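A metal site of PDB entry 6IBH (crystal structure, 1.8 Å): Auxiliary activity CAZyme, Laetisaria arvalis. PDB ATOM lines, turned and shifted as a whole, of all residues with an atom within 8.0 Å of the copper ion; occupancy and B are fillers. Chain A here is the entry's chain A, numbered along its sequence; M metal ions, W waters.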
ATOM      1  N   HIS A   1     -14.385  10.196 -23.379  1.00  0.00           N
ATOM      2  CA  HIS A   1     -15.570  10.129 -22.497  1.00  0.00           C
ATOM      3  C   HIS A   1     -15.139  10.548 -21.086  1.00  0.00           C
ATOM      4  O   HIS A   1     -13.940  10.655 -20.815  1.00  0.00           O
ATOM      5  CB  HIS A   1     -16.140   8.723 -22.486  1.00  0.00           C
ATOM      6  CG  HIS A   1     -16.857   8.408 -23.752  1.00  0.00           C
ATOM      7  ND1 HIS A   1     -16.248   8.526 -25.009  1.00  0.00           N
ATOM      8  CD2 HIS A   1     -18.138   8.043 -23.949  1.00  0.00           C
ATOM      9  CE1 HIS A   1     -17.157   8.179 -25.932  1.00  0.00           C
ATOM     10  NE2 HIS A   1     -18.301   7.853 -25.287  1.00  0.00           N
ATOM     11  N   PHE A   2     -16.105  10.765 -20.190  1.00  0.00           N
ATOM     12  CA  PHE A   2     -15.758  11.348 -18.876  1.00  0.00           C
ATOM     13  C   PHE A   2     -16.723  10.864 -17.795  1.00  0.00           C
ATOM     14  O   PHE A   2     -17.875  10.513 -18.037  1.00  0.00           O
ATOM     15  CB  PHE A   2     -15.693  12.865 -18.929  1.00  0.00           C
ATOM     16  CG  PHE A   2     -17.029  13.547 -18.906  1.00  0.00           C
ATOM     17  CD1 PHE A   2     -17.835  13.548 -20.043  1.00  0.00           C
ATOM     18  CD2 PHE A   2     -17.494  14.141 -17.732  1.00  0.00           C
ATOM     19  CE1 PHE A   2     -19.061  14.177 -19.992  1.00  0.00           C
ATOM     20  CE2 PHE A   2     -18.739  14.751 -17.698  1.00  0.00           C
ATOM     21  CZ  PHE A   2     -19.525  14.743 -18.835  1.00  0.00           C
ATOM     22  N   PHE A  13     -22.227   5.900 -14.668  1.00  0.00           N
ATOM     23  CA  PHE A  13     -21.589   6.201 -15.903  1.00  0.00           C
ATOM     24  C   PHE A  13     -21.822   5.052 -16.876  1.00  0.00           C
ATOM     25  O   PHE A  13     -21.538   3.902 -16.553  1.00  0.00           O
ATOM     26  CB  PHE A  13     -20.088   6.410 -15.697  1.00  0.00           C
ATOM     27  CG  PHE A  13     -19.275   6.319 -16.969  1.00  0.00           C
ATOM     28  CD1 PHE A  13     -19.211   7.387 -17.833  1.00  0.00           C
ATOM     29  CD2 PHE A  13     -18.578   5.166 -17.299  1.00  0.00           C
ATOM     30  CE1 PHE A  13     -18.454   7.321 -18.990  1.00  0.00           C
ATOM     31  CE2 PHE A  13     -17.842   5.088 -18.460  1.00  0.00           C
ATOM     32  CZ  PHE A  13     -17.769   6.172 -19.316  1.00  0.00           C
ATOM     33  N   ALA A  15     -20.844   4.638 -20.927  1.00  0.00           N
ATOM     34  CA  ALA A  15     -20.112   5.353 -21.985  1.00  0.00           C
ATOM     35  C   ALA A  15     -21.052   5.664 -23.173  1.00  0.00           C
ATOM     36  O   ALA A  15     -21.125   6.808 -23.647  1.00  0.00           O
ATOM     37  CB  ALA A  15     -18.922   4.536 -22.409  1.00  0.00           C
ATOM     38  N   GLU A  18     -23.663   8.527 -22.890  1.00  0.00           N
ATOM     39  CA  GLU A  18     -23.240   9.917 -22.673  1.00  0.00           C
ATOM     40  C   GLU A  18     -23.689  10.837 -23.801  1.00  0.00           C
ATOM     41  O   GLU A  18     -23.732  12.027 -23.628  1.00  0.00           O
ATOM     42  CB  GLU A  18     -21.739   9.986 -22.411  1.00  0.00           C
ATOM     43  CG  GLU A  18     -21.348   9.417 -21.064  1.00  0.00           C
ATOM     44  CD  GLU A  18     -20.070  10.011 -20.512  1.00  0.00           C
ATOM     45  OE1 GLU A  18     -19.115  10.176 -21.309  1.00  0.00           O
ATOM     46  OE2 GLU A  18     -20.019  10.315 -19.289  1.00  0.00           O
ATOM     47  N   SER A  47     -11.358  12.407 -17.461  1.00  0.00           N
ATOM     48  CA  SER A  47     -11.443  12.124 -18.900  1.00  0.00           C
ATOM     49  C   SER A  47     -10.517  10.944 -19.263  1.00  0.00           C
ATOM     50  O   SER A  47      -9.370  10.924 -18.870  1.00  0.00           O
ATOM     51  CB  SER A  47     -11.067  13.322 -19.707  1.00  0.00           C
ATOM     52  OG  SER A  47     -11.240  13.080 -21.124  1.00  0.00           O
ATOM     53  N   GLY A  48     -10.996  10.093 -20.145  1.00  0.00           N
ATOM     54  CA  GLY A  48     -10.208   9.016 -20.717  1.00  0.00           C
ATOM     55  C   GLY A  48      -9.222   9.461 -21.792  1.00  0.00           C
ATOM     56  O   GLY A  48      -8.313   8.713 -22.100  1.00  0.00           O
ATOM     57  N   HIS A  49      -9.377  10.673 -22.346  1.00  0.00           N
ATOM     58  CA  HIS A  49      -8.555  11.114 -23.474  1.00  0.00           C
ATOM     59  C   HIS A  49      -8.548  12.624 -23.556  1.00  0.00           C
ATOM     60  O   HIS A  49      -9.361  13.313 -22.922  1.00  0.00           O
ATOM     61  CB  HIS A  49      -8.976  10.446 -24.795  1.00  0.00           C
ATOM     62  CG  HIS A  49     -10.438  10.529 -25.146  1.00  0.00           C
ATOM     63  ND1 HIS A  49     -10.945  11.519 -25.940  1.00  0.00           N
ATOM     64  CD2 HIS A  49     -11.465   9.697 -24.872  1.00  0.00           C
ATOM     65  CE1 HIS A  49     -12.239  11.318 -26.113  1.00  0.00           C
ATOM     66  NE2 HIS A  49     -12.586  10.219 -25.450  1.00  0.00           N
ATOM     67  N   ALA A  50      -7.563  13.153 -24.280  1.00  0.00           N
ATOM     68  CA  ALA A  50      -7.395  14.598 -24.450  1.00  0.00           C
ATOM     69  C   ALA A  50      -6.705  14.821 -25.790  1.00  0.00           C
ATOM     70  O   ALA A  50      -6.038  13.905 -26.239  1.00  0.00           O
ATOM     71  CB  ALA A  50      -6.574  15.157 -23.320  1.00  0.00           C
ATOM     72  N   TYR A  52      -9.826  17.771 -25.088  1.00  0.00           N
ATOM     73  CA  TYR A  52     -11.261  17.851 -25.113  1.00  0.00           C
ATOM     74  C   TYR A  52     -11.646  19.265 -24.672  1.00  0.00           C
ATOM     75  O   TYR A  52     -10.820  20.012 -24.152  1.00  0.00           O
ATOM     76  CB  TYR A  52     -11.912  16.812 -24.204  1.00  0.00           C
ATOM     77  CG  TYR A  52     -11.596  16.936 -22.737  1.00  0.00           C
ATOM     78  CD1 TYR A  52     -10.515  16.271 -22.180  1.00  0.00           C
ATOM     79  CD2 TYR A  52     -12.412  17.653 -21.878  1.00  0.00           C
ATOM     80  CE1 TYR A  52     -10.242  16.336 -20.817  1.00  0.00           C
ATOM     81  CE2 TYR A  52     -12.172  17.709 -20.516  1.00  0.00           C
ATOM     82  CZ  TYR A  52     -11.084  17.040 -19.979  1.00  0.00           C
ATOM     83  OH  TYR A  52     -10.837  17.113 -18.633  1.00  0.00           O
ATOM     84  N   TYR A 118     -19.211  18.064 -22.788  1.00  0.00           N
ATOM     85  CA  TYR A 118     -17.892  17.644 -23.126  1.00  0.00           C
ATOM     86  C   TYR A 118     -17.877  17.278 -24.612  1.00  0.00           C
ATOM     87  O   TYR A 118     -18.797  16.637 -25.088  1.00  0.00           O
ATOM     88  CB  TYR A 118     -17.597  16.387 -22.312  1.00  0.00           C
ATOM     89  CG  TYR A 118     -16.342  15.612 -22.596  1.00  0.00           C
ATOM     90  CD1 TYR A 118     -16.262  14.731 -23.678  1.00  0.00           C
ATOM     91  CD2 TYR A 118     -15.273  15.643 -21.703  1.00  0.00           C
ATOM     92  CE1 TYR A 118     -15.173  13.902 -23.854  1.00  0.00           C
ATOM     93  CE2 TYR A 118     -14.171  14.833 -21.878  1.00  0.00           C
ATOM     94  CZ  TYR A 118     -14.117  13.959 -22.951  1.00  0.00           C
ATOM     95  OH  TYR A 118     -13.032  13.167 -23.146  1.00  0.00           O
ATOM     96  N   THR A 119     -16.821  17.672 -25.329  1.00  0.00           N
ATOM     97  CA  THR A 119     -16.528  17.079 -26.609  1.00  0.00           C
ATOM     98  C   THR A 119     -15.015  16.843 -26.749  1.00  0.00           C
ATOM     99  O   THR A 119     -14.210  17.803 -26.655  1.00  0.00           O
ATOM    100  CB  THR A 119     -17.158  17.937 -27.715  1.00  0.00           C
ATOM    101  OG1 THR A 119     -16.936  17.177 -28.894  1.00  0.00           O
ATOM    102  CG2 THR A 119     -16.628  19.344 -27.828  1.00  0.00           C
ATOM    103  N   GLY A 120     -14.693  15.599 -27.087  1.00  0.00           N
ATOM    104  CA  GLY A 120     -13.389  14.989 -27.079  1.00  0.00           C
ATOM    105  C   GLY A 120     -13.066  14.282 -28.400  1.00  0.00           C
ATOM    106  O   GLY A 120     -12.136  13.510 -28.476  1.00  0.00           O
ATOM    107  N   GLY A 121     -13.892  14.537 -29.423  1.00  0.00           N
ATOM    108  CA  GLY A 121     -13.781  13.936 -30.757  1.00  0.00           C
ATOM    109  C   GLY A 121     -14.664  12.710 -30.974  1.00  0.00           C
ATOM    110  O   GLY A 121     -14.674  12.151 -32.099  1.00  0.00           O
ATOM    111  N   ASP A 122     -15.395  12.268 -29.944  1.00  0.00           N
ATOM    112  CA  ASP A 122     -16.249  11.083 -30.032  1.00  0.00           C
ATOM    113  C   ASP A 122     -17.665  11.392 -29.539  1.00  0.00           C
ATOM    114  O   ASP A 122     -18.261  10.587 -28.888  1.00  0.00           O
ATOM    115  CB  ASP A 122     -15.676   9.843 -29.332  1.00  0.00           C
ATOM    116  CG  ASP A 122     -15.281   9.987 -27.856  1.00  0.00           C
ATOM    117  OD1 ASP A 122     -15.491  11.113 -27.281  1.00  0.00           O
ATOM    118  OD2 ASP A 122     -14.736   8.970 -27.275  1.00  0.00           O
ATOM    119  N   GLY A 123     -18.153  12.571 -29.923  1.00  0.00           N
ATOM    120  CA  GLY A 123     -19.503  13.003 -29.764  1.00  0.00           C
ATOM    121  C   GLY A 123     -19.622  14.155 -28.788  1.00  0.00           C
ATOM    122  O   GLY A 123     -18.621  14.593 -28.139  1.00  0.00           O
ATOM    123  N   LEU A 125     -21.012  14.912 -25.344  1.00  0.00           N
ATOM    124  CA  LEU A 125     -21.261  14.036 -24.220  1.00  0.00           C
ATOM    125  C   LEU A 125     -21.687  14.843 -22.974  1.00  0.00           C
ATOM    126  O   LEU A 125     -21.246  15.961 -22.790  1.00  0.00           O
ATOM    127  CB  LEU A 125     -19.982  13.242 -23.937  1.00  0.00           C
ATOM    128  CG  LEU A 125     -19.378  12.457 -25.105  1.00  0.00           C
ATOM    129  CD1 LEU A 125     -18.205  11.601 -24.660  1.00  0.00           C
ATOM    130  CD2 LEU A 125     -20.422  11.614 -25.783  1.00  0.00           C
HETATM  131 CU    CU M   1     -14.432   9.395 -25.259  1.00  0.00          CU
HETATM  132  O   HOH W   1     -13.522   7.001 -24.571  1.00  0.00           O
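ND1 of His 49 sits close to O of Gly 120 (3.4 Å).
O of Ala 15 lies close to NE2 of His 1 (3.4 Å).
N of His 1 sits close to OH of Tyr 118.
O of His 49 sits at hydrogen-bond distance from OG of Ser 47 (2.6 Å).
The backbone NH (N) of Gly 48 sits at hydrogen-bond distance from the backbone carbonyl oxygen (O) of His 1.
The nearest printed residue that does not touch the copper ion is Leu 125 (4.4 Å).
The copper ion is bound by ND1 of His 1 (2.0 Å), NE2 of His 49 (2.0 Å), N of His 1 (2.0 Å) and OD2 of Asp 122 (2.1 Å).
The copper ion has four donor atoms within binding distance.
Slightly farther from the copper ion lies water W1 (2.7 Å).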
